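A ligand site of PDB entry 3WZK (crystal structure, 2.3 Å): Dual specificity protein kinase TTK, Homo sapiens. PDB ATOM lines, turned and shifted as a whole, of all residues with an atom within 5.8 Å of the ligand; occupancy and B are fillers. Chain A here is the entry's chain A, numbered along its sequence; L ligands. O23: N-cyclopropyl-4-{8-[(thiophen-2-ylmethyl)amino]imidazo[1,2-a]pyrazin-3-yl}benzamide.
NZ of Lys 39 lies within salt-bridge range of OE2 of Glu 57 (3.1 Å).
The backbone carbonyl oxygen (O) of Lys 39 is in hydrogen-bond range of the backbone NH (N) of Met 86, at 2.8 Å.
N of Ile 17 sits at hydrogen-bond distance from O of Val 25.
The backbone carbonyl oxygen (O) of Ala 37 sits at hydrogen-bond distance from the backbone NH (N) of Met 88 (2.8 Å).
The side-chain sulfur (SG) of Cys 90 lies within hydrogen-bond range of the side-chain amide oxygen (OE1) of Gln 27.
The backbone carbonyl oxygen (O) of Lys 15 sits at hydrogen-bond distance from the backbone NH (N) of Gln 27, at 2.8 Å.
The backbone carbonyl oxygen (O) of Ile 149 lies within hydrogen-bond range of a nitrogen (N) of the ligand, 2.6 Å away.
The side-chain amino group (NZ) of Lys 39 lies within hydrogen-bond range of an oxygen (O) of the ligand (3.0 Å).
The backbone NH (N) of Gly 91 lies within hydrogen-bond range of a nitrogen (N1) of the ligand, 3.0 Å away.
The backbone carbonyl oxygen of Gly 91 is in hydrogen-bond range of a nitrogen (N4) of the ligand.
The side-chain amide oxygen (OE1) of Gln 27 sits close to a sulfur (S) of the ligand (3.5 Å).
Lys 15 touches the ligand.
Ile 17 touches the ligand (CG2 to C20, 3.2 Å).
Val 25 touches the ligand (CG2 to C5, 3.9 Å).
CB of Ala 37 touches C11 of the ligand, at 3.5 Å.
Glu 57 touches the ligand.
Leu 61 touches the ligand.
Met 88 touches the ligand.
Glu 89 touches the ligand.
CA of Cys 90 touches N1 of the ligand, at 3.6 Å.
Asn 92 touches the ligand (O to C16, 3.4 Å).
Ile 93 touches the ligand.
Leu 140 touches the ligand.
CB of Asp 150 touches C1 of the ligand (3.6 Å).
Hydrophobic or aromatic side chains within 4 Å of the ligand: Ile 17, Val 25, Ala 37, Leu 61, Met 88, Leu 140 and Ile 149.
Of the 23 residues printed, 17 come within 4 Å of the ligand.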
ATOM      1  N   LYS A  15     -12.469  26.738 -18.353  1.00  0.00           N
ATOM      2  CA  LYS A  15     -13.837  27.049 -18.678  1.00  0.00           C
ATOM      3  C   LYS A  15     -14.741  26.252 -17.735  1.00  0.00           C
ATOM      4  O   LYS A  15     -14.443  25.103 -17.391  1.00  0.00           O
ATOM      5  CB  LYS A  15     -14.101  26.654 -20.139  1.00  0.00           C
ATOM      6  CG  LYS A  15     -15.411  27.111 -20.748  1.00  0.00           C
ATOM      7  CD  LYS A  15     -15.518  26.614 -22.178  1.00  0.00           C
ATOM      8  N   GLN A  16     -15.829  26.888 -17.298  1.00  0.00           N
ATOM      9  CA  GLN A  16     -16.877  26.185 -16.582  1.00  0.00           C
ATOM     10  C   GLN A  16     -17.845  25.659 -17.621  1.00  0.00           C
ATOM     11  O   GLN A  16     -18.270  26.401 -18.516  1.00  0.00           O
ATOM     12  CB  GLN A  16     -17.595  27.102 -15.578  1.00  0.00           C
ATOM     13  CG  GLN A  16     -18.822  26.444 -14.952  1.00  0.00           C
ATOM     14  CD  GLN A  16     -19.274  27.106 -13.669  1.00  0.00           C
ATOM     15  OE1 GLN A  16     -18.526  27.808 -13.003  1.00  0.00           O
ATOM     16  NE2 GLN A  16     -20.530  26.866 -13.309  1.00  0.00           N
ATOM     17  N   ILE A  17     -18.182  24.389 -17.510  1.00  0.00           N
ATOM     18  CA  ILE A  17     -18.988  23.746 -18.534  1.00  0.00           C
ATOM     19  C   ILE A  17     -20.381  23.338 -18.046  1.00  0.00           C
ATOM     20  O   ILE A  17     -21.243  22.991 -18.838  1.00  0.00           O
ATOM     21  CB  ILE A  17     -18.199  22.631 -19.277  1.00  0.00           C
ATOM     22  CG1 ILE A  17     -17.985  21.385 -18.426  1.00  0.00           C
ATOM     23  CG2 ILE A  17     -16.840  23.174 -19.707  1.00  0.00           C
ATOM     24  CD1 ILE A  17     -16.868  20.482 -18.960  1.00  0.00           C
ATOM     25  N   VAL A  25     -19.030  21.801 -12.917  1.00  0.00           N
ATOM     26  CA  VAL A  25     -18.084  21.026 -13.733  1.00  0.00           C
ATOM     27  C   VAL A  25     -17.222  21.984 -14.531  1.00  0.00           C
ATOM     28  O   VAL A  25     -17.725  22.914 -15.165  1.00  0.00           O
ATOM     29  CB  VAL A  25     -18.782  19.995 -14.672  1.00  0.00           C
ATOM     30  CG1 VAL A  25     -17.748  19.221 -15.481  1.00  0.00           C
ATOM     31  CG2 VAL A  25     -19.584  18.981 -13.882  1.00  0.00           C
ATOM     32  N   GLN A  27     -13.869  22.358 -17.290  1.00  0.00           N
ATOM     33  CA  GLN A  27     -12.809  21.883 -18.189  1.00  0.00           C
ATOM     34  C   GLN A  27     -11.495  22.475 -17.697  1.00  0.00           C
ATOM     35  O   GLN A  27     -11.404  23.684 -17.456  1.00  0.00           O
ATOM     36  CB  GLN A  27     -13.100  22.345 -19.623  1.00  0.00           C
ATOM     37  CG  GLN A  27     -12.081  21.949 -20.671  1.00  0.00           C
ATOM     38  CD  GLN A  27     -12.414  22.497 -22.069  1.00  0.00           C
ATOM     39  OE1 GLN A  27     -12.473  21.750 -23.035  1.00  0.00           O
ATOM     40  NE2 GLN A  27     -12.667  23.798 -22.155  1.00  0.00           N
ATOM     41  N   ALA A  37     -12.247  16.929 -17.376  1.00  0.00           N
ATOM     42  CA  ALA A  37     -13.355  17.601 -16.731  1.00  0.00           C
ATOM     43  C   ALA A  37     -13.337  17.239 -15.254  1.00  0.00           C
ATOM     44  O   ALA A  37     -13.410  16.070 -14.898  1.00  0.00           O
ATOM     45  CB  ALA A  37     -14.685  17.220 -17.379  1.00  0.00           C
ATOM     46  N   LYS A  39     -15.406  17.655 -11.754  1.00  0.00           N
ATOM     47  CA  LYS A  39     -16.641  18.022 -11.055  1.00  0.00           C
ATOM     48  C   LYS A  39     -16.326  18.334  -9.588  1.00  0.00           C
ATOM     49  O   LYS A  39     -15.670  17.554  -8.890  1.00  0.00           O
ATOM     50  CB  LYS A  39     -17.659  16.876 -11.144  1.00  0.00           C
ATOM     51  CG  LYS A  39     -19.021  17.174 -10.527  1.00  0.00           C
ATOM     52  CD  LYS A  39     -19.891  15.944 -10.668  1.00  0.00           C
ATOM     53  CE  LYS A  39     -21.323  16.189 -10.249  1.00  0.00           C
ATOM     54  NZ  LYS A  39     -22.122  14.959 -10.511  1.00  0.00           N
ATOM     55  N   GLU A  57     -23.257   7.584  -6.433  1.00  0.00           N
ATOM     56  CA  GLU A  57     -22.794   7.924  -7.779  1.00  0.00           C
ATOM     57  C   GLU A  57     -21.304   7.567  -8.005  1.00  0.00           C
ATOM     58  O   GLU A  57     -20.947   6.931  -8.985  1.00  0.00           O
ATOM     59  CB  GLU A  57     -23.030   9.425  -8.043  1.00  0.00           C
ATOM     60  CG  GLU A  57     -22.948   9.873  -9.497  1.00  0.00           C
ATOM     61  CD  GLU A  57     -23.190  11.384  -9.676  1.00  0.00           C
ATOM     62  OE1 GLU A  57     -24.208  11.753 -10.303  1.00  0.00           O
ATOM     63  OE2 GLU A  57     -22.373  12.207  -9.173  1.00  0.00           O
ATOM     64  N   LEU A  61     -19.883   4.735 -10.502  1.00  0.00           N
ATOM     65  CA  LEU A  61     -18.985   5.158 -11.579  1.00  0.00           C
ATOM     66  C   LEU A  61     -17.638   4.443 -11.516  1.00  0.00           C
ATOM     67  O   LEU A  61     -17.125   4.021 -12.538  1.00  0.00           O
ATOM     68  CB  LEU A  61     -18.813   6.685 -11.589  1.00  0.00           C
ATOM     69  CG  LEU A  61     -18.010   7.280 -12.759  1.00  0.00           C
ATOM     70  CD1 LEU A  61     -18.609   6.921 -14.106  1.00  0.00           C
ATOM     71  CD2 LEU A  61     -17.859   8.797 -12.617  1.00  0.00           C
ATOM     72  N   ILE A  72     -18.335   7.211 -19.159  1.00  0.00           N
ATOM     73  CA  ILE A  72     -17.276   8.194 -18.919  1.00  0.00           C
ATOM     74  C   ILE A  72     -16.194   7.607 -17.998  1.00  0.00           C
ATOM     75  O   ILE A  72     -16.513   6.925 -17.010  1.00  0.00           O
ATOM     76  CB  ILE A  72     -17.852   9.510 -18.309  1.00  0.00           C
ATOM     77  CG1 ILE A  72     -16.840  10.646 -18.370  1.00  0.00           C
ATOM     78  CG2 ILE A  72     -18.354   9.321 -16.879  1.00  0.00           C
ATOM     79  CD1 ILE A  72     -16.931  11.458 -19.647  1.00  0.00           C
ATOM     80  N   MET A  86     -14.168  15.183  -8.702  1.00  0.00           N
ATOM     81  CA  MET A  86     -14.057  14.030  -9.573  1.00  0.00           C
ATOM     82  C   MET A  86     -13.298  14.450 -10.814  1.00  0.00           C
ATOM     83  O   MET A  86     -13.729  15.358 -11.527  1.00  0.00           O
ATOM     84  CB  MET A  86     -15.441  13.460  -9.931  1.00  0.00           C
ATOM     85  CG  MET A  86     -16.299  13.155  -8.713  1.00  0.00           C
ATOM     86  SD  MET A  86     -17.935  12.517  -9.089  1.00  0.00           S
ATOM     87  CE  MET A  86     -18.914  13.358  -7.856  1.00  0.00           C
ATOM     88  N   MET A  88     -12.562  13.431 -14.379  1.00  0.00           N
ATOM     89  CA  MET A  88     -13.153  12.605 -15.402  1.00  0.00           C
ATOM     90  C   MET A  88     -12.643  13.017 -16.777  1.00  0.00           C
ATOM     91  O   MET A  88     -11.961  14.037 -16.911  1.00  0.00           O
ATOM     92  CB  MET A  88     -14.672  12.719 -15.342  1.00  0.00           C
ATOM     93  CG  MET A  88     -15.266  12.216 -14.025  1.00  0.00           C
ATOM     94  SD  MET A  88     -17.006  12.583 -13.930  1.00  0.00           S
ATOM     95  CE  MET A  88     -16.971  14.334 -13.552  1.00  0.00           C
ATOM     96  N   GLU A  89     -12.968  12.198 -17.768  1.00  0.00           N
ATOM     97  CA  GLU A  89     -12.796  12.508 -19.176  1.00  0.00           C
ATOM     98  C   GLU A  89     -13.524  13.797 -19.567  1.00  0.00           C
ATOM     99  O   GLU A  89     -14.647  14.056 -19.115  1.00  0.00           O
ATOM    100  CB  GLU A  89     -13.402  11.369 -20.016  1.00  0.00           C
ATOM    101  CG  GLU A  89     -12.410  10.430 -20.647  1.00  0.00           C
ATOM    102  CD  GLU A  89     -13.072   9.429 -21.582  1.00  0.00           C
ATOM    103  OE1 GLU A  89     -14.027   8.748 -21.166  1.00  0.00           O
ATOM    104  OE2 GLU A  89     -12.627   9.323 -22.732  1.00  0.00           O
ATOM    105  N   CYS A  90     -12.890  14.594 -20.412  1.00  0.00           N
ATOM    106  CA  CYS A  90     -13.564  15.718 -21.037  1.00  0.00           C
ATOM    107  C   CYS A  90     -13.982  15.321 -22.429  1.00  0.00           C
ATOM    108  O   CYS A  90     -13.171  14.784 -23.184  1.00  0.00           O
ATOM    109  CB  CYS A  90     -12.645  16.951 -21.093  1.00  0.00           C
ATOM    110  SG  CYS A  90     -13.550  18.436 -21.584  1.00  0.00           S
ATOM    111  N   GLY A  91     -15.220  15.581 -22.775  1.00  0.00           N
ATOM    112  CA  GLY A  91     -15.676  15.307 -24.137  1.00  0.00           C
ATOM    113  C   GLY A  91     -15.468  16.472 -25.075  1.00  0.00           C
ATOM    114  O   GLY A  91     -15.168  17.585 -24.638  1.00  0.00           O
ATOM    115  N   ASN A  92     -15.623  16.209 -26.369  1.00  0.00           N
ATOM    116  CA  ASN A  92     -15.608  17.272 -27.375  1.00  0.00           C
ATOM    117  C   ASN A  92     -16.883  18.101 -27.279  1.00  0.00           C
ATOM    118  O   ASN A  92     -16.834  19.315 -27.144  1.00  0.00           O
ATOM    119  CB  ASN A  92     -15.440  16.707 -28.787  1.00  0.00           C
ATOM    120  CG  ASN A  92     -14.616  15.428 -28.835  1.00  0.00           C
ATOM    121  OD1 ASN A  92     -14.960  14.494 -29.553  1.00  0.00           O
ATOM    122  ND2 ASN A  92     -13.526  15.370 -28.057  1.00  0.00           N
ATOM    123  N   ILE A  93     -18.033  17.427 -27.320  1.00  0.00           N
ATOM    124  CA  ILE A  93     -19.340  18.087 -27.268  1.00  0.00           C
ATOM    125  C   ILE A  93     -20.410  17.115 -26.729  1.00  0.00           C
ATOM    126  O   ILE A  93     -20.361  15.916 -26.996  1.00  0.00           O
ATOM    127  CB  ILE A  93     -19.712  18.631 -28.680  1.00  0.00           C
ATOM    128  CG1 ILE A  93     -20.936  19.549 -28.632  1.00  0.00           C
ATOM    129  CG2 ILE A  93     -19.863  17.499 -29.706  1.00  0.00           C
ATOM    130  CD1 ILE A  93     -21.265  20.201 -29.966  1.00  0.00           C
ATOM    131  N   ASP A  94     -21.376  17.634 -25.963  1.00  0.00           N
ATOM    132  CA  ASP A  94     -22.499  16.799 -25.541  1.00  0.00           C
ATOM    133  C   ASP A  94     -23.387  16.480 -26.727  1.00  0.00           C
ATOM    134  O   ASP A  94     -23.256  17.100 -27.779  1.00  0.00           O
ATOM    135  CB  ASP A  94     -23.241  17.351 -24.308  1.00  0.00           C
ATOM    136  CG  ASP A  94     -24.218  18.464 -24.626  1.00  0.00           C
ATOM    137  OD1 ASP A  94     -25.275  18.202 -25.236  1.00  0.00           O
ATOM    138  OD2 ASP A  94     -23.966  19.609 -24.206  1.00  0.00           O
ATOM    139  N   LEU A 140     -22.105  11.939 -24.290  1.00  0.00           N
ATOM    140  CA  LEU A 140     -21.001  12.804 -24.612  1.00  0.00           C
ATOM    141  C   LEU A 140     -20.201  12.173 -25.721  1.00  0.00           C
ATOM    142  O   LEU A 140     -20.039  10.963 -25.738  1.00  0.00           O
ATOM    143  CB  LEU A 140     -20.139  12.972 -23.356  1.00  0.00           C
ATOM    144  CG  LEU A 140     -18.969  13.935 -23.334  1.00  0.00           C
ATOM    145  CD1 LEU A 140     -19.454  15.373 -23.453  1.00  0.00           C
ATOM    146  CD2 LEU A 140     -18.210  13.724 -22.040  1.00  0.00           C
ATOM    147  N   ILE A 149     -22.673   9.755 -19.323  1.00  0.00           N
ATOM    148  CA  ILE A 149     -21.899  10.530 -18.340  1.00  0.00           C
ATOM    149  C   ILE A 149     -22.415  10.421 -16.921  1.00  0.00           C
ATOM    150  O   ILE A 149     -21.758  10.879 -15.990  1.00  0.00           O
ATOM    151  CB  ILE A 149     -21.734  12.009 -18.746  1.00  0.00           C
ATOM    152  CG1 ILE A 149     -23.008  12.823 -18.501  1.00  0.00           C
ATOM    153  CG2 ILE A 149     -21.273  12.105 -20.196  1.00  0.00           C
ATOM    154  CD1 ILE A 149     -22.909  14.279 -18.920  1.00  0.00           C
ATOM    155  N   ASP A 150     -23.578   9.814 -16.735  1.00  0.00           N
ATOM    156  CA  ASP A 150     -24.140   9.660 -15.388  1.00  0.00           C
ATOM    157  C   ASP A 150     -25.241   8.602 -15.347  1.00  0.00           C
ATOM    158  O   ASP A 150     -25.539   7.965 -16.355  1.00  0.00           O
ATOM    159  CB  ASP A 150     -24.678  11.004 -14.874  1.00  0.00           C
ATOM    160  CG  ASP A 150     -25.913  11.464 -15.616  1.00  0.00           C
ATOM    161  OD1 ASP A 150     -26.870  11.950 -14.970  1.00  0.00           O
ATOM    162  OD2 ASP A 150     -25.936  11.322 -16.851  1.00  0.00           O
ATOM    163  N   PHE A 151     -25.869   8.453 -14.189  1.00  0.00           N
ATOM    164  CA  PHE A 151     -26.692   7.279 -13.910  1.00  0.00           C
ATOM    165  C   PHE A 151     -28.067   7.614 -13.352  1.00  0.00           C
ATOM    166  O   PHE A 151     -28.820   6.705 -12.979  1.00  0.00           O
ATOM    167  CB  PHE A 151     -25.968   6.374 -12.904  1.00  0.00           C
ATOM    168  CG  PHE A 151     -24.578   6.009 -13.319  1.00  0.00           C
ATOM    169  CD1 PHE A 151     -24.324   5.459 -14.575  1.00  0.00           C
ATOM    170  CD2 PHE A 151     -23.509   6.196 -12.446  1.00  0.00           C
ATOM    171  CE1 PHE A 151     -23.036   5.101 -14.955  1.00  0.00           C
ATOM    172  CE2 PHE A 151     -22.214   5.848 -12.821  1.00  0.00           C
ATOM    173  CZ  PHE A 151     -21.981   5.304 -14.076  1.00  0.00           C
ATOM    174  N   MET A 157     -26.620  17.833 -14.123  1.00  0.00           N
ATOM    175  CA  MET A 157     -25.985  19.134 -14.362  1.00  0.00           C
ATOM    176  C   MET A 157     -26.687  19.891 -15.494  1.00  0.00           C
ATOM    177  O   MET A 157     -27.054  19.294 -16.510  1.00  0.00           O
ATOM    178  CB  MET A 157     -24.500  18.945 -14.703  1.00  0.00           C
ATOM    179  CG  MET A 157     -23.661  18.257 -13.622  1.00  0.00           C
ATOM    180  SD  MET A 157     -23.337  19.295 -12.175  1.00  0.00           S
ATOM    181  CE  MET A 157     -22.152  20.457 -12.837  1.00  0.00           C
HETATM  182  O   O23 L   1     -21.426  14.755 -13.411  1.00  0.00           O
HETATM  183  C   O23 L   1     -21.068  14.006 -14.310  1.00  0.00           C
HETATM  184  N   O23 L   1     -21.251  12.683 -14.212  1.00  0.00           N
HETATM  185  C1  O23 L   1     -21.778  12.135 -12.973  1.00  0.00           C
HETATM  186  C3  O23 L   1     -21.377  10.671 -12.774  1.00  0.00           C
HETATM  187  C2  O23 L   1     -20.611  11.776 -12.055  1.00  0.00           C
HETATM  188  C4  O23 L   1     -20.396  14.601 -15.526  1.00  0.00           C
HETATM  189  C9  O23 L   1     -19.446  13.856 -16.234  1.00  0.00           C
HETATM  190  C8  O23 L   1     -18.826  14.401 -17.364  1.00  0.00           C
HETATM  191  C7  O23 L   1     -19.152  15.695 -17.799  1.00  0.00           C
HETATM  192  C6  O23 L   1     -20.084  16.431 -17.079  1.00  0.00           C
HETATM  193  C5  O23 L   1     -20.718  15.885 -15.946  1.00  0.00           C
HETATM  194  C10 O23 L   1     -18.447  16.232 -19.016  1.00  0.00           C
HETATM  195  N2  O23 L   1     -19.094  17.058 -19.869  1.00  0.00           N
HETATM  196  C13 O23 L   1     -20.340  17.608 -19.921  1.00  0.00           C
HETATM  197  C14 O23 L   1     -20.716  18.479 -20.968  1.00  0.00           C
HETATM  198  N3  O23 L   1     -19.861  18.795 -21.970  1.00  0.00           N
HETATM  199  C15 O23 L   1     -18.610  18.278 -21.955  1.00  0.00           C
HETATM  200  C12 O23 L   1     -18.210  17.352 -20.843  1.00  0.00           C
HETATM  201  N1  O23 L   1     -17.039  16.709 -20.617  1.00  0.00           N
HETATM  202  C11 O23 L   1     -17.160  15.990 -19.469  1.00  0.00           C
HETATM  203  N4  O23 L   1     -17.693  18.552 -22.915  1.00  0.00           N
HETATM  204  C16 O23 L   1     -17.962  19.494 -23.977  1.00  0.00           C
HETATM  205  C17 O23 L   1     -17.599  20.902 -23.558  1.00  0.00           C
HETATM  206  S   O23 L   1     -15.912  21.205 -23.264  1.00  0.00           S
HETATM  207  C20 O23 L   1     -16.155  22.882 -22.854  1.00  0.00           C
HETATM  208  C19 O23 L   1     -17.529  23.134 -22.965  1.00  0.00           C
HETATM  209  C18 O23 L   1     -18.341  22.059 -23.348  1.00  0.00           C
